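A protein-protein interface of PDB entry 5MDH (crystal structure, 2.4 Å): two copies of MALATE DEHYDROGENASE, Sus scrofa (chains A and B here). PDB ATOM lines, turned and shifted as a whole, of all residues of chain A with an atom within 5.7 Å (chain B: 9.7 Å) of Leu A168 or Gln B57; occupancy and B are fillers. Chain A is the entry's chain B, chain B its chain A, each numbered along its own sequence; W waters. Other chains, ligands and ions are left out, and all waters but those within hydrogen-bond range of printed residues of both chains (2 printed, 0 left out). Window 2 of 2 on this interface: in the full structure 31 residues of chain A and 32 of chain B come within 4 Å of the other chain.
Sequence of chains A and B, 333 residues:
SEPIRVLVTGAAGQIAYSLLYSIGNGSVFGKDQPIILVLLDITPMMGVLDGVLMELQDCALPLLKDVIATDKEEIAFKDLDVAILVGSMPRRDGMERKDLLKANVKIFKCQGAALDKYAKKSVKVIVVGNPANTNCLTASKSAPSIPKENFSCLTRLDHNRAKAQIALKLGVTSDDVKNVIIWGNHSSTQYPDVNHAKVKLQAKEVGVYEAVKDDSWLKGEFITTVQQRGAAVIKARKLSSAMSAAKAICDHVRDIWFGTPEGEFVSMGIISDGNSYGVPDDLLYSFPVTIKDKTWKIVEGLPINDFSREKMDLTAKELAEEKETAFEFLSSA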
ATOM      1  N   LYS A 163      22.983   4.670  -9.989  1.00  0.00           N
ATOM      2  CA  LYS A 163      23.058   3.238  -9.705  1.00  0.00           C
ATOM      3  C   LYS A 163      22.536   2.913  -8.305  1.00  0.00           C
ATOM      4  O   LYS A 163      21.778   1.948  -8.104  1.00  0.00           O
ATOM      5  CB  LYS A 163      24.476   2.692  -9.826  1.00  0.00           C
ATOM      6  CG  LYS A 163      24.853   2.304 -11.248  1.00  0.00           C
ATOM      7  CD  LYS A 163      26.345   2.348 -11.506  1.00  0.00           C
ATOM      8  CE  LYS A 163      27.066   1.115 -11.017  1.00  0.00           C
ATOM      9  NZ  LYS A 163      28.504   1.182 -11.376  1.00  0.00           N
ATOM     10  N   ALA A 164      22.968   3.712  -7.331  1.00  0.00           N
ATOM     11  CA  ALA A 164      22.529   3.513  -5.930  1.00  0.00           C
ATOM     12  C   ALA A 164      21.037   3.698  -5.809  1.00  0.00           C
ATOM     13  O   ALA A 164      20.350   2.917  -5.166  1.00  0.00           O
ATOM     14  CB  ALA A 164      23.239   4.460  -4.985  1.00  0.00           C
ATOM     15  N   GLN A 165      20.490   4.701  -6.520  1.00  0.00           N
ATOM     16  CA  GLN A 165      19.026   4.861  -6.484  1.00  0.00           C
ATOM     17  C   GLN A 165      18.273   3.667  -7.041  1.00  0.00           C
ATOM     18  O   GLN A 165      17.295   3.220  -6.427  1.00  0.00           O
ATOM     19  CB  GLN A 165      18.615   6.157  -7.168  1.00  0.00           C
ATOM     20  CG  GLN A 165      19.008   7.374  -6.338  1.00  0.00           C
ATOM     21  CD  GLN A 165      18.491   7.264  -4.921  1.00  0.00           C
ATOM     22  OE1 GLN A 165      17.304   7.069  -4.712  1.00  0.00           O
ATOM     23  NE2 GLN A 165      19.327   7.380  -3.905  1.00  0.00           N
ATOM     24  N   ILE A 166      18.690   3.111  -8.166  1.00  0.00           N
ATOM     25  CA  ILE A 166      18.107   1.923  -8.761  1.00  0.00           C
ATOM     26  C   ILE A 166      18.245   0.750  -7.799  1.00  0.00           C
ATOM     27  O   ILE A 166      17.331  -0.050  -7.610  1.00  0.00           O
ATOM     28  CB  ILE A 166      18.791   1.555 -10.098  1.00  0.00           C
ATOM     29  CG1 ILE A 166      18.570   2.573 -11.208  1.00  0.00           C
ATOM     30  CG2 ILE A 166      18.310   0.183 -10.564  1.00  0.00           C
ATOM     31  CD1 ILE A 166      17.172   2.990 -11.529  1.00  0.00           C
ATOM     32  N   ALA A 167      19.421   0.602  -7.186  1.00  0.00           N
ATOM     33  CA  ALA A 167      19.673  -0.444  -6.203  1.00  0.00           C
ATOM     34  C   ALA A 167      18.723  -0.328  -5.002  1.00  0.00           C
ATOM     35  O   ALA A 167      18.119  -1.313  -4.564  1.00  0.00           O
ATOM     36  CB  ALA A 167      21.112  -0.392  -5.757  1.00  0.00           C
ATOM     37  N   LEU A 168      18.557   0.870  -4.490  1.00  0.00           N
ATOM     38  CA  LEU A 168      17.644   1.181  -3.411  1.00  0.00           C
ATOM     39  C   LEU A 168      16.196   0.876  -3.750  1.00  0.00           C
ATOM     40  O   LEU A 168      15.464   0.245  -2.987  1.00  0.00           O
ATOM     41  CB  LEU A 168      17.783   2.676  -3.032  1.00  0.00           C
ATOM     42  CG  LEU A 168      19.032   3.006  -2.209  1.00  0.00           C
ATOM     43  CD1 LEU A 168      19.046   4.473  -1.779  1.00  0.00           C
ATOM     44  CD2 LEU A 168      19.160   2.089  -0.995  1.00  0.00           C
ATOM     45  N   LYS A 169      15.746   1.319  -4.924  1.00  0.00           N
ATOM     46  CA  LYS A 169      14.379   1.109  -5.377  1.00  0.00           C
ATOM     47  C   LYS A 169      14.040  -0.376  -5.425  1.00  0.00           C
ATOM     48  O   LYS A 169      12.940  -0.730  -5.003  1.00  0.00           O
ATOM     49  CB  LYS A 169      14.173   1.644  -6.797  1.00  0.00           C
ATOM     50  CG  LYS A 169      12.895   1.296  -7.486  1.00  0.00           C
ATOM     51  CD  LYS A 169      11.664   1.493  -6.617  1.00  0.00           C
ATOM     52  CE  LYS A 169      10.892   2.764  -6.883  1.00  0.00           C
ATOM     53  NZ  LYS A 169       9.872   2.912  -5.804  1.00  0.00           N
ATOM     54  N   LEU A 170      14.972  -1.125  -6.026  1.00  0.00           N
ATOM     55  CA  LEU A 170      14.716  -2.548  -6.196  1.00  0.00           C
ATOM     56  C   LEU A 170      15.003  -3.422  -4.984  1.00  0.00           C
ATOM     57  O   LEU A 170      14.442  -4.523  -4.951  1.00  0.00           O
ATOM     58  CB  LEU A 170      15.554  -3.071  -7.378  1.00  0.00           C
ATOM     59  CG  LEU A 170      15.194  -2.489  -8.742  1.00  0.00           C
ATOM     60  CD1 LEU A 170      16.164  -3.025  -9.803  1.00  0.00           C
ATOM     61  CD2 LEU A 170      13.735  -2.827  -9.073  1.00  0.00           C
ATOM     62  N   GLY A 171      15.938  -3.029  -4.129  1.00  0.00           N
ATOM     63  CA  GLY A 171      16.350  -3.887  -3.019  1.00  0.00           C
ATOM     64  C   GLY A 171      17.551  -4.734  -3.446  1.00  0.00           C
ATOM     65  O   GLY A 171      17.834  -5.813  -2.936  1.00  0.00           O
ATOM     66  N   VAL A 172      18.325  -4.207  -4.376  1.00  0.00           N
ATOM     67  CA  VAL A 172      19.515  -4.913  -4.910  1.00  0.00           C
ATOM     68  C   VAL A 172      20.766  -4.085  -4.643  1.00  0.00           C
ATOM     69  O   VAL A 172      20.787  -3.008  -4.019  1.00  0.00           O
ATOM     70  CB  VAL A 172      19.135  -5.110  -6.403  1.00  0.00           C
ATOM     71  CG1 VAL A 172      19.984  -4.319  -7.376  1.00  0.00           C
ATOM     72  CG2 VAL A 172      19.002  -6.559  -6.846  1.00  0.00           C
ATOM     73  N   SER A 174      24.371  -1.901  -5.655  1.00  0.00           N
ATOM     74  CA  SER A 174      24.684  -0.871  -6.628  1.00  0.00           C
ATOM     75  C   SER A 174      25.470  -1.458  -7.773  1.00  0.00           C
ATOM     76  O   SER A 174      25.144  -1.166  -8.924  1.00  0.00           O
ATOM     77  CB  SER A 174      25.305   0.376  -5.977  1.00  0.00           C
ATOM     78  OG  SER A 174      26.413   0.791  -6.744  1.00  0.00           O
ATOM     79  N   ARG A 229      20.482  15.216  -5.417  1.00  0.00           N
ATOM     80  CA  ARG A 229      21.253  14.497  -4.441  1.00  0.00           C
ATOM     81  C   ARG A 229      22.373  15.290  -3.772  1.00  0.00           C
ATOM     82  O   ARG A 229      22.516  15.125  -2.547  1.00  0.00           O
ATOM     83  CB  ARG A 229      21.855  13.194  -5.020  1.00  0.00           C
ATOM     84  CG  ARG A 229      22.512  12.345  -3.952  1.00  0.00           C
ATOM     85  CD  ARG A 229      21.531  11.648  -3.019  1.00  0.00           C
ATOM     86  NE  ARG A 229      22.181  10.461  -2.462  1.00  0.00           N
ATOM     87  CZ  ARG A 229      21.494   9.560  -1.755  1.00  0.00           C
ATOM     88  NH1 ARG A 229      20.183   9.736  -1.522  1.00  0.00           N
ATOM     89  NH2 ARG A 229      22.146   8.480  -1.303  1.00  0.00           N
ATOM     90  N   LEU B  20      35.071   5.864   7.677  1.00  0.00           N
ATOM     91  CA  LEU B  20      33.973   4.945   7.346  1.00  0.00           C
ATOM     92  C   LEU B  20      34.148   4.291   5.990  1.00  0.00           C
ATOM     93  O   LEU B  20      33.834   3.089   5.908  1.00  0.00           O
ATOM     94  CB  LEU B  20      32.580   5.569   7.535  1.00  0.00           C
ATOM     95  CG  LEU B  20      32.453   6.363   8.836  1.00  0.00           C
ATOM     96  CD1 LEU B  20      31.067   6.967   9.069  1.00  0.00           C
ATOM     97  CD2 LEU B  20      32.900   5.513  10.011  1.00  0.00           C
ATOM     98  N   TYR B  21      34.624   5.027   4.976  1.00  0.00           N
ATOM     99  CA  TYR B  21      34.849   4.432   3.672  1.00  0.00           C
ATOM    100  C   TYR B  21      35.772   3.202   3.686  1.00  0.00           C
ATOM    101  O   TYR B  21      35.484   2.174   3.055  1.00  0.00           O
ATOM    102  CB  TYR B  21      35.484   5.482   2.742  1.00  0.00           C
ATOM    103  CG  TYR B  21      35.739   4.883   1.368  1.00  0.00           C
ATOM    104  CD1 TYR B  21      34.647   4.479   0.615  1.00  0.00           C
ATOM    105  CD2 TYR B  21      37.005   4.716   0.842  1.00  0.00           C
ATOM    106  CE1 TYR B  21      34.822   3.904  -0.632  1.00  0.00           C
ATOM    107  CE2 TYR B  21      37.196   4.138  -0.405  1.00  0.00           C
ATOM    108  CZ  TYR B  21      36.113   3.752  -1.139  1.00  0.00           C
ATOM    109  OH  TYR B  21      36.217   3.179  -2.381  1.00  0.00           O
ATOM    110  N   GLY B  24      33.810   0.098   5.380  1.00  0.00           N
ATOM    111  CA  GLY B  24      32.793  -0.351   4.453  1.00  0.00           C
ATOM    112  C   GLY B  24      33.307  -0.986   3.186  1.00  0.00           C
ATOM    113  O   GLY B  24      32.591  -1.788   2.577  1.00  0.00           O
ATOM    114  N   LEU B  37      27.352  -1.635  10.746  1.00  0.00           N
ATOM    115  CA  LEU B  37      28.048  -0.427  11.175  1.00  0.00           C
ATOM    116  C   LEU B  37      27.202   0.410  12.120  1.00  0.00           C
ATOM    117  O   LEU B  37      26.109   0.808  11.700  1.00  0.00           O
ATOM    118  CB  LEU B  37      28.400   0.394   9.933  1.00  0.00           C
ATOM    119  CG  LEU B  37      29.680   1.185   9.839  1.00  0.00           C
ATOM    120  CD1 LEU B  37      29.493   2.510   9.068  1.00  0.00           C
ATOM    121  CD2 LEU B  37      30.389   1.395  11.165  1.00  0.00           C
ATOM    122  N   LEU B  49      24.808  12.880  10.365  1.00  0.00           N
ATOM    123  CA  LEU B  49      24.865  11.430  10.205  1.00  0.00           C
ATOM    124  C   LEU B  49      24.090  10.990   8.979  1.00  0.00           C
ATOM    125  O   LEU B  49      24.710  10.386   8.083  1.00  0.00           O
ATOM    126  CB  LEU B  49      24.474  10.763  11.511  1.00  0.00           C
ATOM    127  CG  LEU B  49      25.445   9.760  12.123  1.00  0.00           C
ATOM    128  CD1 LEU B  49      26.891  10.213  11.912  1.00  0.00           C
ATOM    129  CD2 LEU B  49      25.198   9.560  13.597  1.00  0.00           C
ATOM    130  N   ASP B  50      22.836  11.368   8.794  1.00  0.00           N
ATOM    131  CA  ASP B  50      22.025  11.108   7.632  1.00  0.00           C
ATOM    132  C   ASP B  50      22.708  11.521   6.333  1.00  0.00           C
ATOM    133  O   ASP B  50      22.493  10.851   5.290  1.00  0.00           O
ATOM    134  CB  ASP B  50      20.645  11.763   7.720  1.00  0.00           C
ATOM    135  CG  ASP B  50      19.722  11.322   8.836  1.00  0.00           C
ATOM    136  OD1 ASP B  50      19.709  10.149   9.291  1.00  0.00           O
ATOM    137  OD2 ASP B  50      18.914  12.159   9.358  1.00  0.00           O
ATOM    138  N   GLY B  51      23.484  12.596   6.280  1.00  0.00           N
ATOM    139  CA  GLY B  51      24.228  12.966   5.071  1.00  0.00           C
ATOM    140  C   GLY B  51      25.326  11.933   4.799  1.00  0.00           C
ATOM    141  O   GLY B  51      25.529  11.487   3.661  1.00  0.00           O
ATOM    142  N   VAL B  52      26.026  11.516   5.864  1.00  0.00           N
ATOM    143  CA  VAL B  52      27.029  10.452   5.783  1.00  0.00           C
ATOM    144  C   VAL B  52      26.370   9.160   5.319  1.00  0.00           C
ATOM    145  O   VAL B  52      26.866   8.494   4.431  1.00  0.00           O
ATOM    146  CB  VAL B  52      27.683  10.255   7.164  1.00  0.00           C
ATOM    147  CG1 VAL B  52      28.664   9.111   7.202  1.00  0.00           C
ATOM    148  CG2 VAL B  52      28.415  11.545   7.553  1.00  0.00           C
ATOM    149  N   LEU B  53      25.149   8.819   5.774  1.00  0.00           N
ATOM    150  CA  LEU B  53      24.543   7.591   5.308  1.00  0.00           C
ATOM    151  C   LEU B  53      24.279   7.628   3.802  1.00  0.00           C
ATOM    152  O   LEU B  53      24.697   6.646   3.163  1.00  0.00           O
ATOM    153  CB  LEU B  53      23.338   7.058   6.044  1.00  0.00           C
ATOM    154  CG  LEU B  53      23.385   6.865   7.548  1.00  0.00           C
ATOM    155  CD1 LEU B  53      22.393   5.779   7.962  1.00  0.00           C
ATOM    156  CD2 LEU B  53      24.774   6.663   8.135  1.00  0.00           C
ATOM    157  N   MET B  54      23.756   8.738   3.282  1.00  0.00           N
ATOM    158  CA  MET B  54      23.525   8.833   1.845  1.00  0.00           C
ATOM    159  C   MET B  54      24.844   8.709   1.086  1.00  0.00           C
ATOM    160  O   MET B  54      24.909   8.091   0.030  1.00  0.00           O
ATOM    161  CB  MET B  54      22.839  10.151   1.462  1.00  0.00           C
ATOM    162  CG  MET B  54      21.407  10.393   1.952  1.00  0.00           C
ATOM    163  SD  MET B  54      20.953  12.154   1.731  1.00  0.00           S
ATOM    164  CE  MET B  54      19.302  11.840   1.120  1.00  0.00           C
ATOM    165  N   GLU B  55      25.931   9.271   1.587  1.00  0.00           N
ATOM    166  CA  GLU B  55      27.224   9.146   0.945  1.00  0.00           C
ATOM    167  C   GLU B  55      27.704   7.687   1.014  1.00  0.00           C
ATOM    168  O   GLU B  55      28.243   7.174   0.031  1.00  0.00           O
ATOM    169  CB  GLU B  55      28.305  10.047   1.523  1.00  0.00           C
ATOM    170  CG  GLU B  55      27.980  11.524   1.428  1.00  0.00           C
ATOM    171  CD  GLU B  55      29.263  12.336   1.346  1.00  0.00           C
ATOM    172  OE1 GLU B  55      29.971  12.230   0.313  1.00  0.00           O
ATOM    173  OE2 GLU B  55      29.595  13.044   2.280  1.00  0.00           O
ATOM    174  N   LEU B  56      27.449   6.984   2.108  1.00  0.00           N
ATOM    175  CA  LEU B  56      27.864   5.561   2.106  1.00  0.00           C
ATOM    176  C   LEU B  56      27.095   4.808   1.015  1.00  0.00           C
ATOM    177  O   LEU B  56      27.670   4.039   0.251  1.00  0.00           O
ATOM    178  CB  LEU B  56      27.659   4.931   3.492  1.00  0.00           C
ATOM    179  CG  LEU B  56      28.512   5.634   4.571  1.00  0.00           C
ATOM    180  CD1 LEU B  56      28.014   5.250   5.942  1.00  0.00           C
ATOM    181  CD2 LEU B  56      29.983   5.235   4.395  1.00  0.00           C
ATOM    182  N   GLN B  57      25.800   5.072   0.827  1.00  0.00           N
ATOM    183  CA  GLN B  57      25.034   4.416  -0.216  1.00  0.00           C
ATOM    184  C   GLN B  57      25.572   4.798  -1.586  1.00  0.00           C
ATOM    185  O   GLN B  57      25.593   3.962  -2.493  1.00  0.00           O
ATOM    186  CB  GLN B  57      23.536   4.682  -0.195  1.00  0.00           C
ATOM    187  CG  GLN B  57      22.719   4.379   1.025  1.00  0.00           C
ATOM    188  CD  GLN B  57      21.373   5.063   1.061  1.00  0.00           C
ATOM    189  OE1 GLN B  57      21.138   6.077   0.399  1.00  0.00           O
ATOM    190  NE2 GLN B  57      20.426   4.544   1.835  1.00  0.00           N
ATOM    191  N   ASP B  58      26.110   6.018  -1.726  1.00  0.00           N
ATOM    192  CA  ASP B  58      26.638   6.496  -3.008  1.00  0.00           C
ATOM    193  C   ASP B  58      28.057   6.051  -3.289  1.00  0.00           C
ATOM    194  O   ASP B  58      28.588   6.309  -4.378  1.00  0.00           O
ATOM    195  CB  ASP B  58      26.519   8.026  -3.043  1.00  0.00           C
ATOM    196  CG  ASP B  58      25.052   8.429  -3.052  1.00  0.00           C
ATOM    197  OD1 ASP B  58      24.235   7.495  -3.267  1.00  0.00           O
ATOM    198  OD2 ASP B  58      24.736   9.606  -2.810  1.00  0.00           O
ATOM    199  N   CYS B  59      28.677   5.365  -2.325  1.00  0.00           N
ATOM    200  CA  CYS B  59      30.002   4.820  -2.480  1.00  0.00           C
ATOM    201  C   CYS B  59      30.033   3.357  -2.929  1.00  0.00           C
ATOM    202  O   CYS B  59      31.132   2.833  -3.119  1.00  0.00           O
ATOM    203  CB  CYS B  59      30.790   4.955  -1.174  1.00  0.00           C
ATOM    204  SG  CYS B  59      31.293   6.655  -0.850  1.00  0.00           S
ATOM    205  N   ALA B  60      28.916   2.701  -3.164  1.00  0.00           N
ATOM    206  CA  ALA B  60      28.900   1.303  -3.615  1.00  0.00           C
ATOM    207  C   ALA B  60      29.546   0.382  -2.599  1.00  0.00           C
ATOM    208  O   ALA B  60      30.549  -0.269  -2.913  1.00  0.00           O
ATOM    209  CB  ALA B  60      29.594   1.136  -4.971  1.00  0.00           C
ATOM    210  N   LEU B  61      29.015   0.245  -1.382  1.00  0.00           N
ATOM    211  CA  LEU B  61      29.663  -0.617  -0.391  1.00  0.00           C
ATOM    212  C   LEU B  61      28.762  -1.753   0.049  1.00  0.00           C
ATOM    213  O   LEU B  61      28.037  -1.611   1.034  1.00  0.00           O
ATOM    214  CB  LEU B  61      30.078   0.230   0.826  1.00  0.00           C
ATOM    215  CG  LEU B  61      30.971   1.445   0.526  1.00  0.00           C
ATOM    216  CD1 LEU B  61      30.841   2.532   1.593  1.00  0.00           C
ATOM    217  CD2 LEU B  61      32.418   1.028   0.321  1.00  0.00           C
ATOM    218  N   PRO B  62      28.765  -2.878  -0.667  1.00  0.00           N
ATOM    219  CA  PRO B  62      27.906  -4.008  -0.379  1.00  0.00           C
ATOM    220  C   PRO B  62      28.199  -4.734   0.915  1.00  0.00           C
ATOM    221  O   PRO B  62      27.288  -5.342   1.521  1.00  0.00           O
ATOM    222  CB  PRO B  62      28.080  -4.942  -1.596  1.00  0.00           C
ATOM    223  CG  PRO B  62      29.376  -4.553  -2.248  1.00  0.00           C
ATOM    224  CD  PRO B  62      29.616  -3.111  -1.871  1.00  0.00           C
ATOM    225  N   LEU B  64      28.472  -3.424   3.653  1.00  0.00           N
ATOM    226  CA  LEU B  64      27.725  -2.742   4.700  1.00  0.00           C
ATOM    227  C   LEU B  64      26.343  -3.365   4.807  1.00  0.00           C
ATOM    228  O   LEU B  64      25.397  -2.999   4.136  1.00  0.00           O
ATOM    229  CB  LEU B  64      27.693  -1.234   4.533  1.00  0.00           C
ATOM    230  CG  LEU B  64      28.961  -0.460   4.913  1.00  0.00           C
ATOM    231  CD1 LEU B  64      28.743   1.024   4.639  1.00  0.00           C
ATOM    232  CD2 LEU B  64      29.375  -0.693   6.358  1.00  0.00           C
ATOM    233  N   ASP B  66      24.197  -3.167   7.290  1.00  0.00           N
ATOM    234  CA  ASP B  66      23.264  -2.220   7.866  1.00  0.00           C
ATOM    235  C   ASP B  66      24.102  -1.086   8.430  1.00  0.00           C
ATOM    236  O   ASP B  66      25.282  -1.314   8.678  1.00  0.00           O
ATOM    237  CB  ASP B  66      22.445  -2.894   8.985  1.00  0.00           C
ATOM    238  CG  ASP B  66      21.131  -2.202   9.292  1.00  0.00           C
ATOM    239  OD1 ASP B  66      20.743  -1.266   8.566  1.00  0.00           O
ATOM    240  OD2 ASP B  66      20.436  -2.572  10.261  1.00  0.00           O
ATOM    241  N   VAL B  67      23.521   0.103   8.502  1.00  0.00           N
ATOM    242  CA  VAL B  67      24.179   1.275   9.043  1.00  0.00           C
ATOM    243  C   VAL B  67      23.201   1.954  10.025  1.00  0.00           C
ATOM    244  O   VAL B  67      22.153   2.445   9.615  1.00  0.00           O
ATOM    245  CB  VAL B  67      24.607   2.334   8.008  1.00  0.00           C
ATOM    246  CG1 VAL B  67      25.447   3.406   8.707  1.00  0.00           C
ATOM    247  CG2 VAL B  67      25.348   1.782   6.792  1.00  0.00           C
HETATM  248  O   HOH W   1      18.367   7.524  -0.713  1.00  0.00           O
HETATM  249  O   HOH W   2      21.838   8.392  -4.882  1.00  0.00           O
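OE1 of Gln B57 is in hydrogen-bond range of NH2 of Arg A229.
O of Met B54 is in hydrogen-bond range of NH2 of Arg A229.
The guanidinium group of Arg A229 is in salt-bridge range of the side-chain carboxylate of Asp B58 (2.7 Å).
The side-chain amide nitrogen (NE2) of Gln A165 lies close to the guanidinium group (NH1) of Arg A229, 3.5 Å away.
Among the printed residues, merely in contact across the chains: Leu A168 with Gln B57 (3.4 Å), Ala A164 with Gln B57 (3.5 Å), Ala A164 with Asp B58 (3.6 Å) and Ser A174 with Ala B60 (3.7 Å).
Of chain B, only Gln B57 and Asp B58 come within 4 Å of Ala A164.
No residue of chain B comes within 4 Å of Ala A167.
Of chain B, only Gln B57 comes within 4 Å of Leu A168.
Leu A170 touches none of the printed residues of chain B.
Printed residues of chain B within 4 Å of Ser A174: Ala B60 (3.7 Å).
Of the printed residues of chain B, Arg A229 touches Met B54 (3.1 Å), Gln B57 (3.1 Å) and Asp B58 (2.7 Å).
Of the printed residues of chain A, Met B54 touches Arg A229 (3.1 Å).
Gln B57 touches just these residues of chain A: Ala A164 (3.5 Å), Leu A168 (3.4 Å) and Arg A229 (3.1 Å).
Printed residues of chain A within 4 Å of Ala B60: Ser A174 (3.7 Å).
The nearest residue of chain A that does not touch Gln B57 is Gln A165 (4.8 Å).
The nearest printed residue of chain A that does not touch Asp B58 is Gln A165 (5.0 Å).
Of the 12 printed residues of chain A, 4 touch a printed residue of chain B.
Printed residues of chain A that touch a printed residue of chain B: Ala A164, Leu A168, Ser A174 and Arg A229.
Hydrophobic or aromatic side chains of chain A within 4 Å of the printed part of chain B: Ala A164 and Leu A168.
Hydrophobic or aromatic side chains of chain B within 4 Å of the printed part of chain A: Met B54 and Ala B60.
Among the printed residues, 7 pairs touch across the chains.
Among the printed residues, Asp or Glu carboxylates within 4 Å of a Lys or Arg side-chain nitrogen of the other chain: Arg A229 with Asp B58.
No position is printed for both chains.
Of the 7 pairs that touch across the chains among the printed residues, none has its exchanged pair printed and touching as well.
Water W2 lies within hydrogen-bond range of the side-chain amide nitrogen of Gln A165 (2.9 Å), the side-chain carboxylate of Asp B58 (3.0 Å) and the guanidinium group of Arg A229 (3.2 Å).
Water W1 lies within hydrogen-bond range of NH1 of Arg A229, OE1 of Gln B57 and NE2 of Gln A165.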
